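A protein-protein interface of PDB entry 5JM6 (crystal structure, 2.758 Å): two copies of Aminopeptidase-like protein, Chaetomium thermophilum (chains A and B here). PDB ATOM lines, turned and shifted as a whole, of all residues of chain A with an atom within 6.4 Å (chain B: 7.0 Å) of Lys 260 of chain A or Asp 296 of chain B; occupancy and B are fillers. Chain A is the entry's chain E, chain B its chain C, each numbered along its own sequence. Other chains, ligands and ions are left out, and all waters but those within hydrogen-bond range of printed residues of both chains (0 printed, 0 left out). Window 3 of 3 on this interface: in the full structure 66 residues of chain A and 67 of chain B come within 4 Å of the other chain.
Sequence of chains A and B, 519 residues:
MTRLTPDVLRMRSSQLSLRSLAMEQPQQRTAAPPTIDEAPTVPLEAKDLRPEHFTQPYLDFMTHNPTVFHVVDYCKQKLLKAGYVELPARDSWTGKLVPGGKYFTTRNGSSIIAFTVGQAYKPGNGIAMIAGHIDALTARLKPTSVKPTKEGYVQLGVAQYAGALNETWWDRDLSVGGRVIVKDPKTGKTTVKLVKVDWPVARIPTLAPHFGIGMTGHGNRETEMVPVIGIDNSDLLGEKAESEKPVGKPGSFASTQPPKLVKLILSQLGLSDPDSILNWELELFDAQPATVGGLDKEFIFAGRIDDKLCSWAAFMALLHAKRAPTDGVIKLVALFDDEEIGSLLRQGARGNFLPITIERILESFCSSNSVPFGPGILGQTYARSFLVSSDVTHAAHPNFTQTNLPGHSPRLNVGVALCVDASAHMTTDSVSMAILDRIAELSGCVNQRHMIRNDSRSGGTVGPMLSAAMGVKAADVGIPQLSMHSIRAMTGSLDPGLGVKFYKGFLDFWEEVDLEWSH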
ATOM      1  N   TRP A 199      15.414 -14.983  -9.965  1.00  0.00           N
ATOM      2  CA  TRP A 199      16.497 -14.230 -10.591  1.00  0.00           C
ATOM      3  C   TRP A 199      16.877 -13.060  -9.690  1.00  0.00           C
ATOM      4  O   TRP A 199      16.053 -12.605  -8.896  1.00  0.00           O
ATOM      5  CB  TRP A 199      16.085 -13.733 -11.979  1.00  0.00           C
ATOM      6  CG  TRP A 199      15.161 -12.559 -11.940  1.00  0.00           C
ATOM      7  CD1 TRP A 199      15.508 -11.243 -11.826  1.00  0.00           C
ATOM      8  CD2 TRP A 199      13.733 -12.592 -12.020  1.00  0.00           C
ATOM      9  NE1 TRP A 199      14.383 -10.456 -11.824  1.00  0.00           N
ATOM     10  CE2 TRP A 199      13.280 -11.260 -11.944  1.00  0.00           C
ATOM     11  CE3 TRP A 199      12.793 -13.619 -12.148  1.00  0.00           C
ATOM     12  CZ2 TRP A 199      11.929 -10.929 -11.991  1.00  0.00           C
ATOM     13  CZ3 TRP A 199      11.452 -13.287 -12.195  1.00  0.00           C
ATOM     14  CH2 TRP A 199      11.033 -11.954 -12.117  1.00  0.00           C
ATOM     15  N   ILE A 229      16.971  -1.856  -7.083  1.00  0.00           N
ATOM     16  CA  ILE A 229      16.108  -2.872  -7.693  1.00  0.00           C
ATOM     17  C   ILE A 229      15.597  -2.644  -9.128  1.00  0.00           C
ATOM     18  O   ILE A 229      14.936  -3.521  -9.686  1.00  0.00           O
ATOM     19  CB  ILE A 229      14.888  -3.116  -6.797  1.00  0.00           C
ATOM     20  CG1 ILE A 229      13.985  -1.885  -6.778  1.00  0.00           C
ATOM     21  CG2 ILE A 229      15.341  -3.476  -5.390  1.00  0.00           C
ATOM     22  CD1 ILE A 229      12.842  -1.994  -5.802  1.00  0.00           C
ATOM     23  N   GLY A 230      15.883  -1.491  -9.724  1.00  0.00           N
ATOM     24  CA  GLY A 230      15.345  -1.193 -11.043  1.00  0.00           C
ATOM     25  C   GLY A 230      15.633   0.220 -11.513  1.00  0.00           C
ATOM     26  O   GLY A 230      16.253   1.005 -10.798  1.00  0.00           O
ATOM     27  N   VAL A 247       0.003   0.526  -5.643  1.00  0.00           N
ATOM     28  CA  VAL A 247      -0.728  -0.679  -6.036  1.00  0.00           C
ATOM     29  C   VAL A 247      -2.051  -0.923  -5.280  1.00  0.00           C
ATOM     30  O   VAL A 247      -2.942  -1.574  -5.818  1.00  0.00           O
ATOM     31  CB  VAL A 247       0.179  -1.925  -5.928  1.00  0.00           C
ATOM     32  CG1 VAL A 247      -0.537  -3.149  -6.407  1.00  0.00           C
ATOM     33  CG2 VAL A 247       1.366  -1.747  -6.818  1.00  0.00           C
ATOM     34  N   GLN A 257       5.019  -0.673  -0.169  1.00  0.00           N
ATOM     35  CA  GLN A 257       6.056  -1.489  -0.793  1.00  0.00           C
ATOM     36  C   GLN A 257       6.294  -1.058  -2.236  1.00  0.00           C
ATOM     37  O   GLN A 257       5.450  -0.379  -2.822  1.00  0.00           O
ATOM     38  CB  GLN A 257       5.662  -2.968  -0.731  1.00  0.00           C
ATOM     39  CG  GLN A 257       5.239  -3.438   0.655  1.00  0.00           C
ATOM     40  CD  GLN A 257       6.411  -3.589   1.607  1.00  0.00           C
ATOM     41  OE1 GLN A 257       7.386  -4.280   1.309  1.00  0.00           O
ATOM     42  NE2 GLN A 257       6.327  -2.930   2.756  1.00  0.00           N
ATOM     43  N   PRO A 258       7.465  -1.407  -2.801  1.00  0.00           N
ATOM     44  CA  PRO A 258       7.689  -1.140  -4.225  1.00  0.00           C
ATOM     45  C   PRO A 258       6.603  -1.786  -5.070  1.00  0.00           C
ATOM     46  O   PRO A 258       6.309  -2.966  -4.874  1.00  0.00           O
ATOM     47  CB  PRO A 258       9.051  -1.783  -4.494  1.00  0.00           C
ATOM     48  CG  PRO A 258       9.737  -1.750  -3.181  1.00  0.00           C
ATOM     49  CD  PRO A 258       8.661  -1.977  -2.158  1.00  0.00           C
ATOM     50  N   PRO A 259       6.005  -1.019  -5.991  1.00  0.00           N
ATOM     51  CA  PRO A 259       4.857  -1.532  -6.739  1.00  0.00           C
ATOM     52  C   PRO A 259       5.162  -2.795  -7.535  1.00  0.00           C
ATOM     53  O   PRO A 259       4.367  -3.732  -7.466  1.00  0.00           O
ATOM     54  CB  PRO A 259       4.498  -0.369  -7.669  1.00  0.00           C
ATOM     55  CG  PRO A 259       5.027   0.837  -6.981  1.00  0.00           C
ATOM     56  CD  PRO A 259       6.302   0.380  -6.337  1.00  0.00           C
ATOM     57  N   LYS A 260       6.277  -2.854  -8.258  1.00  0.00           N
ATOM     58  CA  LYS A 260       6.519  -4.070  -9.022  1.00  0.00           C
ATOM     59  C   LYS A 260       6.862  -5.253  -8.109  1.00  0.00           C
ATOM     60  O   LYS A 260       6.558  -6.398  -8.446  1.00  0.00           O
ATOM     61  CB  LYS A 260       7.611  -3.903 -10.089  1.00  0.00           C
ATOM     62  CG  LYS A 260       7.892  -5.267 -10.714  1.00  0.00           C
ATOM     63  CD  LYS A 260       8.000  -5.402 -12.211  1.00  0.00           C
ATOM     64  CE  LYS A 260       7.759  -6.890 -12.508  1.00  0.00           C
ATOM     65  NZ  LYS A 260       8.699  -7.557 -13.445  1.00  0.00           N
ATOM     66  N   LEU A 261       7.454  -5.002  -6.945  1.00  0.00           N
ATOM     67  CA  LEU A 261       7.700  -6.112  -6.032  1.00  0.00           C
ATOM     68  C   LEU A 261       6.373  -6.763  -5.655  1.00  0.00           C
ATOM     69  O   LEU A 261       6.245  -7.984  -5.690  1.00  0.00           O
ATOM     70  CB  LEU A 261       8.447  -5.663  -4.779  1.00  0.00           C
ATOM     71  CG  LEU A 261       8.797  -6.816  -3.835  1.00  0.00           C
ATOM     72  CD1 LEU A 261       9.649  -7.864  -4.545  1.00  0.00           C
ATOM     73  CD2 LEU A 261       9.501  -6.293  -2.599  1.00  0.00           C
ATOM     74  N   VAL A 262       5.379  -5.941  -5.331  1.00  0.00           N
ATOM     75  CA  VAL A 262       4.061  -6.445  -4.967  1.00  0.00           C
ATOM     76  C   VAL A 262       3.435  -7.269  -6.095  1.00  0.00           C
ATOM     77  O   VAL A 262       2.945  -8.373  -5.859  1.00  0.00           O
ATOM     78  CB  VAL A 262       3.109  -5.299  -4.578  1.00  0.00           C
ATOM     79  CG1 VAL A 262       1.710  -5.830  -4.334  1.00  0.00           C
ATOM     80  CG2 VAL A 262       3.628  -4.586  -3.340  1.00  0.00           C
ATOM     81  N   LYS A 263       3.465  -6.747  -7.317  1.00  0.00           N
ATOM     82  CA  LYS A 263       2.890  -7.469  -8.448  1.00  0.00           C
ATOM     83  C   LYS A 263       3.648  -8.755  -8.729  1.00  0.00           C
ATOM     84  O   LYS A 263       3.057  -9.767  -9.107  1.00  0.00           O
ATOM     85  CB  LYS A 263       2.885  -6.613  -9.707  1.00  0.00           C
ATOM     86  CG  LYS A 263       2.329  -5.225  -9.538  1.00  0.00           C
ATOM     87  CD  LYS A 263       2.165  -4.606 -10.905  1.00  0.00           C
ATOM     88  CE  LYS A 263       2.638  -3.171 -10.955  1.00  0.00           C
ATOM     89  NZ  LYS A 263       2.592  -2.690 -12.364  1.00  0.00           N
ATOM     90  N   LEU A 264       4.963  -8.703  -8.562  1.00  0.00           N
ATOM     91  CA  LEU A 264       5.792  -9.877  -8.776  1.00  0.00           C
ATOM     92  C   LEU A 264       5.429 -10.944  -7.754  1.00  0.00           C
ATOM     93  O   LEU A 264       5.272 -12.113  -8.099  1.00  0.00           O
ATOM     94  CB  LEU A 264       7.274  -9.515  -8.677  1.00  0.00           C
ATOM     95  CG  LEU A 264       8.264 -10.475  -9.333  1.00  0.00           C
ATOM     96  CD1 LEU A 264       8.025 -10.535 -10.833  1.00  0.00           C
ATOM     97  CD2 LEU A 264       9.687 -10.036  -9.029  1.00  0.00           C
ATOM     98  N   ILE A 265       5.270 -10.528  -6.501  1.00  0.00           N
ATOM     99  CA  ILE A 265       4.928 -11.451  -5.424  1.00  0.00           C
ATOM    100  C   ILE A 265       3.519 -12.026  -5.607  1.00  0.00           C
ATOM    101  O   ILE A 265       3.293 -13.207  -5.341  1.00  0.00           O
ATOM    102  CB  ILE A 265       5.049 -10.766  -4.039  1.00  0.00           C
ATOM    103  CG1 ILE A 265       6.501 -10.366  -3.770  1.00  0.00           C
ATOM    104  CG2 ILE A 265       4.582 -11.689  -2.927  1.00  0.00           C
ATOM    105  CD1 ILE A 265       7.471 -11.527  -3.810  1.00  0.00           C
ATOM    106  N   GLY B 293      19.433  -8.602 -14.361  1.00  0.00           N
ATOM    107  CA  GLY B 293      18.866  -8.520 -13.033  1.00  0.00           C
ATOM    108  C   GLY B 293      18.033  -7.275 -12.836  1.00  0.00           C
ATOM    109  O   GLY B 293      17.930  -6.429 -13.726  1.00  0.00           O
ATOM    110  N   GLY B 294      17.456  -7.157 -11.648  1.00  0.00           N
ATOM    111  CA  GLY B 294      16.500  -6.109 -11.362  1.00  0.00           C
ATOM    112  C   GLY B 294      15.109  -6.698 -11.452  1.00  0.00           C
ATOM    113  O   GLY B 294      14.922  -7.773 -12.022  1.00  0.00           O
ATOM    114  N   LEU B 295      14.132  -6.003 -10.883  1.00  0.00           N
ATOM    115  CA  LEU B 295      12.763  -6.494 -10.890  1.00  0.00           C
ATOM    116  C   LEU B 295      12.250  -6.665 -12.315  1.00  0.00           C
ATOM    117  O   LEU B 295      11.500  -7.595 -12.609  1.00  0.00           O
ATOM    118  CB  LEU B 295      11.855  -5.548 -10.108  1.00  0.00           C
ATOM    119  CG  LEU B 295      12.111  -5.524  -8.602  1.00  0.00           C
ATOM    120  CD1 LEU B 295      11.370  -4.368  -7.964  1.00  0.00           C
ATOM    121  CD2 LEU B 295      11.694  -6.844  -7.975  1.00  0.00           C
ATOM    122  N   ASP B 296      12.619  -5.731 -13.181  1.00  0.00           N
ATOM    123  CA  ASP B 296      12.239  -5.782 -14.586  1.00  0.00           C
ATOM    124  C   ASP B 296      13.348  -6.264 -15.532  1.00  0.00           C
ATOM    125  O   ASP B 296      13.203  -6.169 -16.752  1.00  0.00           O
ATOM    126  CB  ASP B 296      11.724  -4.419 -15.027  1.00  0.00           C
ATOM    127  CG  ASP B 296      10.620  -4.528 -16.048  1.00  0.00           C
ATOM    128  OD1 ASP B 296       9.975  -5.596 -16.115  1.00  0.00           O
ATOM    129  OD2 ASP B 296      10.395  -3.544 -16.781  1.00  0.00           O
ATOM    130  N   LYS B 297      14.471  -6.708 -14.968  1.00  0.00           N
ATOM    131  CA  LYS B 297      15.632  -7.153 -15.747  1.00  0.00           C
ATOM    132  C   LYS B 297      16.184  -6.021 -16.610  1.00  0.00           C
ATOM    133  O   LYS B 297      16.519  -6.213 -17.778  1.00  0.00           O
ATOM    134  CB  LYS B 297      15.282  -8.375 -16.605  1.00  0.00           C
ATOM    135  CG  LYS B 297      15.035  -9.623 -15.772  1.00  0.00           C
ATOM    136  CD  LYS B 297      14.470 -10.780 -16.575  1.00  0.00           C
ATOM    137  CE  LYS B 297      14.134 -11.938 -15.644  1.00  0.00           C
ATOM    138  NZ  LYS B 297      13.790 -13.190 -16.371  1.00  0.00           N
ATOM    139  N   GLU B 298      16.283  -4.841 -16.008  1.00  0.00           N
ATOM    140  CA  GLU B 298      16.841  -3.672 -16.678  1.00  0.00           C
ATOM    141  C   GLU B 298      18.360  -3.644 -16.582  1.00  0.00           C
ATOM    142  O   GLU B 298      19.019  -2.892 -17.295  1.00  0.00           O
ATOM    143  CB  GLU B 298      16.278  -2.388 -16.072  1.00  0.00           C
ATOM    144  CG  GLU B 298      14.795  -2.425 -15.788  1.00  0.00           C
ATOM    145  CD  GLU B 298      14.496  -2.683 -14.326  1.00  0.00           C
ATOM    146  OE1 GLU B 298      13.633  -1.974 -13.766  1.00  0.00           O
ATOM    147  OE2 GLU B 298      15.116  -3.596 -13.739  1.00  0.00           O
ATOM    148  N   PHE B 299      18.906  -4.475 -15.699  1.00  0.00           N
ATOM    149  CA  PHE B 299      20.325  -4.443 -15.360  1.00  0.00           C
ATOM    150  C   PHE B 299      21.094  -5.581 -16.006  1.00  0.00           C
ATOM    151  O   PHE B 299      20.531  -6.631 -16.299  1.00  0.00           O
ATOM    152  CB  PHE B 299      20.523  -4.521 -13.844  1.00  0.00           C
ATOM    153  CG  PHE B 299      19.975  -3.347 -13.097  1.00  0.00           C
ATOM    154  CD1 PHE B 299      20.240  -2.059 -13.520  1.00  0.00           C
ATOM    155  CD2 PHE B 299      19.192  -3.532 -11.970  1.00  0.00           C
ATOM    156  CE1 PHE B 299      19.742  -0.979 -12.831  1.00  0.00           C
ATOM    157  CE2 PHE B 299      18.687  -2.453 -11.281  1.00  0.00           C
ATOM    158  CZ  PHE B 299      18.958  -1.173 -11.718  1.00  0.00           C
ATOM    159  N   SER B 493      20.526  -3.115 -19.144  1.00  0.00           N
ATOM    160  CA  SER B 493      20.447  -4.231 -20.081  1.00  0.00           C
ATOM    161  C   SER B 493      20.420  -3.781 -21.543  1.00  0.00           C
ATOM    162  O   SER B 493      20.723  -4.567 -22.441  1.00  0.00           O
ATOM    163  CB  SER B 493      19.217  -5.092 -19.777  1.00  0.00           C
ATOM    164  OG  SER B 493      18.023  -4.340 -19.892  1.00  0.00           O
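O of Leu 295 of chain B sits at hydrogen-bond distance from NZ of Lys 260 of chain A, at 2.9 Å.
The backbone carbonyl oxygen of Ile 229 of chain A sits at hydrogen-bond distance from the backbone NH of Leu 295 of chain B, 2.9 Å away.
The side-chain amino group (NZ) of Lys 260 of chain A lies within salt-bridge range of the side-chain carboxylate (OD1) of Asp 296 of chain B, 3.6 Å away.
The indole nitrogen of Trp 199 of chain A sits at hydrogen-bond distance from the backbone carbonyl oxygen of Gly 294 of chain B (2.7 Å).
Lys 260 of chain A touches two residues of chain B.
Printed residues of chain A within 4 Å of Asp 296 of chain B: Lys 260 (3.6 Å).
Of the printed residues of chain A, Lys 297 of chain B touches Trp 199 (3.7 Å).
Printed residues of chain B within 4 Å of Leu 264 of chain A: Leu 295.
Printed residues of chain A within 4 Å of Gly 294 of chain B: Trp 199 (2.7 Å) and Ile 229 (3.5 Å).
Ser 493 of chain B touches none of the printed residues of chain A.
Lys 263 of chain A touches none of the printed residues of chain B.
The nearest residue of chain B that does not touch Lys 260 of chain A is Lys 297 of chain B (6.0 Å).
The nearest residue of chain A that does not touch Asp 296 of chain B is Ile 229 of chain A (4.7 Å).
No position is printed for both chains.
The backbone NH of Phe 299 of chain B is in hydrogen-bond range of the backbone carbonyl oxygen of Gly 293 of chain B (2.9 Å).
O of Gly 293 of chain B sits at hydrogen-bond distance from N of Glu 298 of chain B, 3.2 Å away.
N of Asp 296 of chain B lies within hydrogen-bond range of OE2 of Glu 298 of chain B (3.3 Å).
OG of Ser 493 of chain B lies within hydrogen-bond range of O of Glu 298 of chain B (3.1 Å).
The backbone carbonyl oxygen (O) of Lys 297 of chain B sits at hydrogen-bond distance from the side-chain hydroxyl (OG) of Ser 493 of chain B, 3.2 Å away.
Among the printed residues, pairs that only touch across the chains: Gly 230 of chain A with Glu 298 of chain B (3.3 Å), Gly 230 of chain A with Phe 299 of chain B (3.3 Å), Trp 199 of chain A with Leu 295 of chain B (3.4 Å), Ile 229 of chain A with Gly 294 of chain B (3.5 Å), Trp 199 of chain A with Lys 297 of chain B (3.7 Å), Ile 229 of chain A with Phe 299 of chain B (3.8 Å) and Leu 264 of chain A with Leu 295 of chain B (3.9 Å).
Hydrophobic or aromatic side chains of chain A within 4 Å of the printed part of chain B: Trp 199, Ile 229 and Leu 264.
Printed residues of chain B that touch a printed residue of chain A: Gly 294, Leu 295, Asp 296, Lys 297, Glu 298 and Phe 299.
Hydrophobic or aromatic side chains of chain B within 4 Å of the printed part of chain A: Leu 295 and Phe 299.
Among the printed residues, 11 pairs touch across the chains.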
